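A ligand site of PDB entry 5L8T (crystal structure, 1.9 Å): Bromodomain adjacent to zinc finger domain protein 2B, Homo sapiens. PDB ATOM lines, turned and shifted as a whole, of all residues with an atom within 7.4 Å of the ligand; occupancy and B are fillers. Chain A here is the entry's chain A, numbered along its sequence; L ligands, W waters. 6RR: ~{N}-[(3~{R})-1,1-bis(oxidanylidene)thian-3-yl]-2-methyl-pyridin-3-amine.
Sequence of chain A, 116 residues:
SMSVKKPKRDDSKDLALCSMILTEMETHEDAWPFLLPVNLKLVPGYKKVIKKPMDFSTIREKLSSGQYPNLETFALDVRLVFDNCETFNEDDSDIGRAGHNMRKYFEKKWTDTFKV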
ATOM      1  N   TRP A  32      22.824  -1.714  22.339  1.00  0.00           N
ATOM      2  CA  TRP A  32      23.759  -0.804  21.683  1.00  0.00           C
ATOM      3  C   TRP A  32      23.203   0.033  20.524  1.00  0.00           C
ATOM      4  O   TRP A  32      23.632   1.183  20.345  1.00  0.00           O
ATOM      5  CB  TRP A  32      25.009  -1.566  21.210  1.00  0.00           C
ATOM      6  CG  TRP A  32      24.723  -2.620  20.211  1.00  0.00           C
ATOM      7  CD1 TRP A  32      24.441  -3.933  20.467  1.00  0.00           C
ATOM      8  CD2 TRP A  32      24.713  -2.484  18.783  1.00  0.00           C
ATOM      9  NE1 TRP A  32      24.244  -4.617  19.291  1.00  0.00           N
ATOM     10  CE2 TRP A  32      24.396  -3.739  18.239  1.00  0.00           C
ATOM     11  CE3 TRP A  32      24.914  -1.402  17.905  1.00  0.00           C
ATOM     12  CZ2 TRP A  32      24.289  -3.965  16.867  1.00  0.00           C
ATOM     13  CZ3 TRP A  32      24.807  -1.620  16.544  1.00  0.00           C
ATOM     14  CH2 TRP A  32      24.500  -2.894  16.037  1.00  0.00           C
ATOM     15  N   PRO A  33      22.241  -0.500  19.737  1.00  0.00           N
ATOM     16  CA  PRO A  33      21.813   0.427  18.674  1.00  0.00           C
ATOM     17  C   PRO A  33      20.959   1.600  19.172  1.00  0.00           C
ATOM     18  O   PRO A  33      20.706   2.533  18.422  1.00  0.00           O
ATOM     19  CB  PRO A  33      20.979  -0.462  17.733  1.00  0.00           C
ATOM     20  CG  PRO A  33      21.353  -1.901  18.107  1.00  0.00           C
ATOM     21  CD  PRO A  33      21.605  -1.825  19.581  1.00  0.00           C
ATOM     22  N   PHE A  34      20.524   1.539  20.433  1.00  0.00           N
ATOM     23  CA  PHE A  34      19.487   2.448  20.925  1.00  0.00           C
ATOM     24  C   PHE A  34      19.927   3.332  22.072  1.00  0.00           C
ATOM     25  O   PHE A  34      19.095   4.038  22.633  1.00  0.00           O
ATOM     26  CB  PHE A  34      18.277   1.640  21.384  1.00  0.00           C
ATOM     27  CG  PHE A  34      17.881   0.573  20.400  1.00  0.00           C
ATOM     28  CD1 PHE A  34      17.329   0.923  19.175  1.00  0.00           C
ATOM     29  CD2 PHE A  34      18.098  -0.761  20.682  1.00  0.00           C
ATOM     30  CE1 PHE A  34      16.984  -0.055  18.245  1.00  0.00           C
ATOM     31  CE2 PHE A  34      17.742  -1.741  19.761  1.00  0.00           C
ATOM     32  CZ  PHE A  34      17.190  -1.396  18.556  1.00  0.00           C
ATOM     33  N   LEU A  35      21.200   3.277  22.427  1.00  0.00           N
ATOM     34  CA  LEU A  35      21.676   3.945  23.615  1.00  0.00           C
ATOM     35  C   LEU A  35      21.720   5.451  23.421  1.00  0.00           C
ATOM     36  O   LEU A  35      21.452   6.196  24.354  1.00  0.00           O
ATOM     37  CB  LEU A  35      23.052   3.425  24.015  1.00  0.00           C
ATOM     38  CG  LEU A  35      23.073   1.959  24.468  1.00  0.00           C
ATOM     39  CD1 LEU A  35      24.502   1.521  24.786  1.00  0.00           C
ATOM     40  CD2 LEU A  35      22.167   1.761  25.675  1.00  0.00           C
ATOM     41  N   LEU A  36      22.059   5.871  22.212  1.00  0.00           N
ATOM     42  CA  LEU A  36      22.215   7.291  21.856  1.00  0.00           C
ATOM     43  C   LEU A  36      21.363   7.621  20.641  1.00  0.00           C
ATOM     44  O   LEU A  36      21.005   6.716  19.881  1.00  0.00           O
ATOM     45  CB  LEU A  36      23.685   7.610  21.585  1.00  0.00           C
ATOM     46  CG  LEU A  36      24.661   7.446  22.750  1.00  0.00           C
ATOM     47  CD1 LEU A  36      26.075   7.793  22.279  1.00  0.00           C
ATOM     48  CD2 LEU A  36      24.250   8.322  23.917  1.00  0.00           C
ATOM     49  N   PRO A  37      21.034   8.897  20.434  1.00  0.00           N
ATOM     50  CA  PRO A  37      20.262   9.261  19.239  1.00  0.00           C
ATOM     51  C   PRO A  37      20.930   8.769  17.964  1.00  0.00           C
ATOM     52  O   PRO A  37      22.161   8.763  17.898  1.00  0.00           O
ATOM     53  CB  PRO A  37      20.252  10.807  19.269  1.00  0.00           C
ATOM     54  CG  PRO A  37      20.460  11.156  20.684  1.00  0.00           C
ATOM     55  CD  PRO A  37      21.344  10.072  21.268  1.00  0.00           C
ATOM     56  N   VAL A  38      20.142   8.340  16.991  1.00  0.00           N
ATOM     57  CA  VAL A  38      20.723   8.040  15.687  1.00  0.00           C
ATOM     58  C   VAL A  38      21.440   9.275  15.186  1.00  0.00           C
ATOM     59  O   VAL A  38      20.895  10.381  15.181  1.00  0.00           O
ATOM     60  CB  VAL A  38      19.666   7.584  14.670  1.00  0.00           C
ATOM     61  CG1 VAL A  38      20.272   7.501  13.275  1.00  0.00           C
ATOM     62  CG2 VAL A  38      19.060   6.245  15.087  1.00  0.00           C
ATOM     63  N   ASN A  39      22.705   9.074  14.817  1.00  0.00           N
ATOM     64  CA  ASN A  39      23.530  10.144  14.268  1.00  0.00           C
ATOM     65  C   ASN A  39      22.991  10.567  12.907  1.00  0.00           C
ATOM     66  O   ASN A  39      23.171   9.868  11.911  1.00  0.00           O
ATOM     67  CB  ASN A  39      24.976   9.672  14.167  1.00  0.00           C
ATOM     68  CG  ASN A  39      25.955  10.811  13.968  1.00  0.00           C
ATOM     69  OD1 ASN A  39      25.662  11.783  13.268  1.00  0.00           O
ATOM     70  ND2 ASN A  39      27.112  10.702  14.595  1.00  0.00           N
ATOM     71  N   LEU A  40      22.348  11.733  12.873  1.00  0.00           N
ATOM     72  CA  LEU A  40      21.606  12.175  11.698  1.00  0.00           C
ATOM     73  C   LEU A  40      22.504  12.558  10.534  1.00  0.00           C
ATOM     74  O   LEU A  40      22.028  12.777   9.424  1.00  0.00           O
ATOM     75  CB  LEU A  40      20.705  13.375  12.046  1.00  0.00           C
ATOM     76  CG  LEU A  40      19.553  13.119  13.029  1.00  0.00           C
ATOM     77  CD1 LEU A  40      18.717  14.376  13.177  1.00  0.00           C
ATOM     78  CD2 LEU A  40      18.696  11.954  12.557  1.00  0.00           C
ATOM     79  N   LEU A  42      25.408  10.680  10.068  1.00  0.00           N
ATOM     80  CA  LEU A  42      26.156   9.457   9.823  1.00  0.00           C
ATOM     81  C   LEU A  42      25.246   8.446   9.139  1.00  0.00           C
ATOM     82  O   LEU A  42      25.706   7.523   8.466  1.00  0.00           O
ATOM     83  CB  LEU A  42      26.693   8.888  11.149  1.00  0.00           C
ATOM     84  CG  LEU A  42      27.595   7.644  11.242  1.00  0.00           C
ATOM     85  CD1 LEU A  42      28.381   7.688  12.535  1.00  0.00           C
ATOM     86  CD2 LEU A  42      26.809   6.352  11.173  1.00  0.00           C
ATOM     87  N   VAL A  43      23.944   8.616   9.336  1.00  0.00           N
ATOM     88  CA  VAL A  43      22.980   7.654   8.837  1.00  0.00           C
ATOM     89  C   VAL A  43      22.078   8.309   7.812  1.00  0.00           C
ATOM     90  O   VAL A  43      21.171   9.045   8.163  1.00  0.00           O
ATOM     91  CB  VAL A  43      22.110   7.071   9.974  1.00  0.00           C
ATOM     92  CG1 VAL A  43      21.106   6.066   9.444  1.00  0.00           C
ATOM     93  CG2 VAL A  43      23.002   6.424  11.012  1.00  0.00           C
ATOM     94  N   TYR A  46      17.832   9.149   7.640  1.00  0.00           N
ATOM     95  CA  TYR A  46      17.105   8.968   8.896  1.00  0.00           C
ATOM     96  C   TYR A  46      16.214  10.158   9.243  1.00  0.00           C
ATOM     97  O   TYR A  46      15.054   9.981   9.638  1.00  0.00           O
ATOM     98  CB  TYR A  46      18.069   8.692  10.055  1.00  0.00           C
ATOM     99  CG  TYR A  46      17.368   7.966  11.182  1.00  0.00           C
ATOM    100  CD1 TYR A  46      16.935   8.653  12.324  1.00  0.00           C
ATOM    101  CD2 TYR A  46      17.081   6.615  11.079  1.00  0.00           C
ATOM    102  CE1 TYR A  46      16.267   7.995  13.335  1.00  0.00           C
ATOM    103  CE2 TYR A  46      16.423   5.948  12.088  1.00  0.00           C
ATOM    104  CZ  TYR A  46      16.020   6.637  13.220  1.00  0.00           C
ATOM    105  OH  TYR A  46      15.352   5.991  14.223  1.00  0.00           O
ATOM    106  N   ILE A  50      12.227   9.339   9.503  1.00  0.00           N
ATOM    107  CA  ILE A  50      11.748   9.090  10.862  1.00  0.00           C
ATOM    108  C   ILE A  50      11.303  10.401  11.505  1.00  0.00           C
ATOM    109  O   ILE A  50      12.126  11.223  11.905  1.00  0.00           O
ATOM    110  CB  ILE A  50      12.822   8.410  11.732  1.00  0.00           C
ATOM    111  CG1 ILE A  50      13.246   7.073  11.113  1.00  0.00           C
ATOM    112  CG2 ILE A  50      12.332   8.232  13.180  1.00  0.00           C
ATOM    113  CD1 ILE A  50      12.096   6.095  10.905  1.00  0.00           C
ATOM    114  N   MET A  54      13.762   8.629  18.685  1.00  0.00           N
ATOM    115  CA  MET A  54      13.811   8.408  20.125  1.00  0.00           C
ATOM    116  C   MET A  54      14.882   7.370  20.425  1.00  0.00           C
ATOM    117  O   MET A  54      15.176   6.499  19.586  1.00  0.00           O
ATOM    118  CB  MET A  54      12.435   7.976  20.649  1.00  0.00           C
ATOM    119  CG  MET A  54      12.344   7.859  22.172  1.00  0.00           C
ATOM    120  SD  MET A  54      12.799   9.390  23.021  1.00  0.00           S
ATOM    121  CE  MET A  54      11.658  10.555  22.277  1.00  0.00           C
ATOM    122  N   VAL A  81      10.900   3.868  20.085  1.00  0.00           N
ATOM    123  CA  VAL A  81      12.251   3.421  19.751  1.00  0.00           C
ATOM    124  C   VAL A  81      12.202   2.205  18.822  1.00  0.00           C
ATOM    125  O   VAL A  81      12.871   2.166  17.799  1.00  0.00           O
ATOM    126  CB  VAL A  81      13.072   3.064  21.000  1.00  0.00           C
ATOM    127  CG1 VAL A  81      14.412   2.457  20.608  1.00  0.00           C
ATOM    128  CG2 VAL A  81      13.262   4.324  21.913  1.00  0.00           C
ATOM    129  N   ASN A  84      10.358   2.901  15.337  1.00  0.00           N
ATOM    130  CA  ASN A  84      11.314   3.533  14.419  1.00  0.00           C
ATOM    131  C   ASN A  84      12.282   2.512  13.837  1.00  0.00           C
ATOM    132  O   ASN A  84      12.555   2.499  12.637  1.00  0.00           O
ATOM    133  CB  ASN A  84      12.105   4.619  15.139  1.00  0.00           C
ATOM    134  CG  ASN A  84      11.265   5.842  15.474  1.00  0.00           C
ATOM    135  OD1 ASN A  84      10.167   6.019  14.947  1.00  0.00           O
ATOM    136  ND2 ASN A  84      11.800   6.699  16.339  1.00  0.00           N
ATOM    137  N   CYS A  85      12.803   1.660  14.715  1.00  0.00           N
ATOM    138  CA  CYS A  85      13.798   0.677  14.317  1.00  0.00           C
ATOM    139  C   CYS A  85      13.226  -0.245  13.250  1.00  0.00           C
ATOM    140  O   CYS A  85      13.900  -0.584  12.279  1.00  0.00           O
ATOM    141  CB  CYS A  85      14.284  -0.113  15.537  1.00  0.00           C
ATOM    142  SG  CYS A  85      15.514  -1.422  15.159  1.00  0.00           S
ATOM    143  N   GLU A  86      11.957  -0.624  13.419  1.00  0.00           N
ATOM    144  CA  GLU A  86      11.322  -1.558  12.493  1.00  0.00           C
ATOM    145  C   GLU A  86      11.037  -0.876  11.158  1.00  0.00           C
ATOM    146  O   GLU A  86      11.068  -1.518  10.100  1.00  0.00           O
ATOM    147  CB  GLU A  86      10.033  -2.114  13.102  1.00  0.00           C
ATOM    148  CG  GLU A  86       9.808  -3.577  12.819  1.00  0.00           C
ATOM    149  CD  GLU A  86       8.587  -4.128  13.534  1.00  0.00           C
ATOM    150  OE1 GLU A  86       8.427  -3.871  14.744  1.00  0.00           O
ATOM    151  OE2 GLU A  86       7.780  -4.817  12.878  1.00  0.00           O
ATOM    152  N   PHE A  88      12.974   1.410   9.825  1.00  0.00           N
ATOM    153  CA  PHE A  88      14.212   1.733   9.117  1.00  0.00           C
ATOM    154  C   PHE A  88      15.122   0.541   8.822  1.00  0.00           C
ATOM    155  O   PHE A  88      15.951   0.607   7.910  1.00  0.00           O
ATOM    156  CB  PHE A  88      15.021   2.770   9.908  1.00  0.00           C
ATOM    157  CG  PHE A  88      15.900   3.630   9.033  1.00  0.00           C
ATOM    158  CD1 PHE A  88      15.358   4.673   8.303  1.00  0.00           C
ATOM    159  CD2 PHE A  88      17.259   3.375   8.930  1.00  0.00           C
ATOM    160  CE1 PHE A  88      16.164   5.459   7.481  1.00  0.00           C
ATOM    161  CE2 PHE A  88      18.065   4.156   8.127  1.00  0.00           C
ATOM    162  CZ  PHE A  88      17.513   5.199   7.398  1.00  0.00           C
ATOM    163  N   ASN A  89      14.963  -0.534   9.580  1.00  0.00           N
ATOM    164  CA  ASN A  89      15.870  -1.666   9.463  1.00  0.00           C
ATOM    165  C   ASN A  89      15.160  -2.948   9.048  1.00  0.00           C
ATOM    166  O   ASN A  89      14.029  -3.210   9.454  1.00  0.00           O
ATOM    167  CB  ASN A  89      16.602  -1.898  10.792  1.00  0.00           C
ATOM    168  CG  ASN A  89      17.400  -0.677  11.246  1.00  0.00           C
ATOM    169  OD1 ASN A  89      18.569  -0.509  10.890  1.00  0.00           O
ATOM    170  ND2 ASN A  89      16.756   0.177  12.042  1.00  0.00           N
ATOM    171  N   ILE A  95      20.690  -4.803  13.583  1.00  0.00           N
ATOM    172  CA  ILE A  95      19.960  -3.766  14.308  1.00  0.00           C
ATOM    173  C   ILE A  95      18.464  -4.095  14.360  1.00  0.00           C
ATOM    174  O   ILE A  95      17.816  -3.937  15.401  1.00  0.00           O
ATOM    175  CB  ILE A  95      20.171  -2.381  13.667  1.00  0.00           C
ATOM    176  CG1 ILE A  95      21.593  -1.910  13.924  1.00  0.00           C
ATOM    177  CG2 ILE A  95      19.164  -1.377  14.193  1.00  0.00           C
ATOM    178  CD1 ILE A  95      21.964  -0.628  13.190  1.00  0.00           C
ATOM    179  N   GLY A  96      17.929  -4.574  13.246  1.00  0.00           N
ATOM    180  CA  GLY A  96      16.534  -4.970  13.192  1.00  0.00           C
ATOM    181  C   GLY A  96      16.190  -6.071  14.197  1.00  0.00           C
ATOM    182  O   GLY A  96      15.177  -5.982  14.894  1.00  0.00           O
HETATM  183  O10 6RR L   1      24.713   4.637  13.348  1.00  0.00           O
HETATM  184  C15 6RR L   1      18.613   3.176  12.245  1.00  0.00           C
HETATM  185  C14 6RR L   1      19.992   3.272  11.878  1.00  0.00           C
HETATM  186  C12 6RR L   1      22.935   4.451  15.177  1.00  0.00           C
HETATM  187  C01 6RR L   1      18.690   2.241  15.890  1.00  0.00           C
HETATM  188  C02 6RR L   1      19.163   2.616  14.438  1.00  0.00           C
HETATM  189  C03 6RR L   1      20.570   2.698  14.170  1.00  0.00           C
HETATM  190  N04 6RR L   1      21.556   2.433  15.240  1.00  0.00           N
HETATM  191  C05 6RR L   1      22.908   2.944  15.032  1.00  0.00           C
HETATM  192  C06 6RR L   1      23.979   2.206  16.011  1.00  0.00           C
HETATM  193  C07 6RR L   1      25.313   3.049  16.438  1.00  0.00           C
HETATM  194  C08 6RR L   1      25.675   4.322  15.660  1.00  0.00           C
HETATM  195  S09 6RR L   1      24.462   5.010  14.718  1.00  0.00           S
HETATM  196  O11 6RR L   1      24.479   6.438  14.854  1.00  0.00           O
HETATM  197  C13 6RR L   1      20.980   3.033  12.840  1.00  0.00           C
HETATM  198  N16 6RR L   1      18.264   2.856  13.508  1.00  0.00           N
HETATM  199  O   HOH W   1      15.805   3.395  14.312  1.00  0.00           O
HETATM  200  O   HOH W   2      23.419   5.876  18.058  1.00  0.00           O
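The backbone NH (N) of Asn 39 is in hydrogen-bond range of an oxygen (O11) of the ligand (3.2 Å).
O of Pro 33 lies close to N04 of the ligand, at 3.3 Å.
ND2 of Asn 89 lies within hydrogen-bond range of N16 of the ligand, at 3.4 Å.
CZ3 of Trp 32 touches C06 of the ligand, at 3.95 Å.
Phe 34 touches the ligand.
Val 38 touches the ligand (CG2 to C02, 3.7 Å).
CD2 of Leu 42 touches O10 of the ligand (3.5 Å).
Val 43 touches the ligand (CG2 to O10, 3.4 Å).
Tyr 46 touches the ligand.
Phe 88 touches the ligand.
CD1 of Ile 95 touches N04 of the ligand, at 3.7 Å.
Hydrophobic or aromatic side chains that line the ligand: Trp 32, Pro 33, Phe 34, Val 38, Leu 42, Val 43, Tyr 46, Phe 88 and Ile 95.
11 residues have an atom within 4 Å of the ligand: Trp 32, Pro 33, Phe 34, Val 38, Asn 39, Leu 42, Val 43, Tyr 46, Phe 88, Asn 89 and Ile 95.
OD1 of Asn 39 is in hydrogen-bond range of N of Leu 42, 3.4 Å away.
ND2 of Asn 89 sits at hydrogen-bond distance from O of Cys 85 (3.0 Å).
O of Ile 95 is in hydrogen-bond range of SG of Cys 85, 3.4 Å away.
Water W1 lies within hydrogen-bond range of OH of Tyr 46 (2.6 Å), N16 of the ligand (2.6 Å) and N of Cys 85 (3.5 Å).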
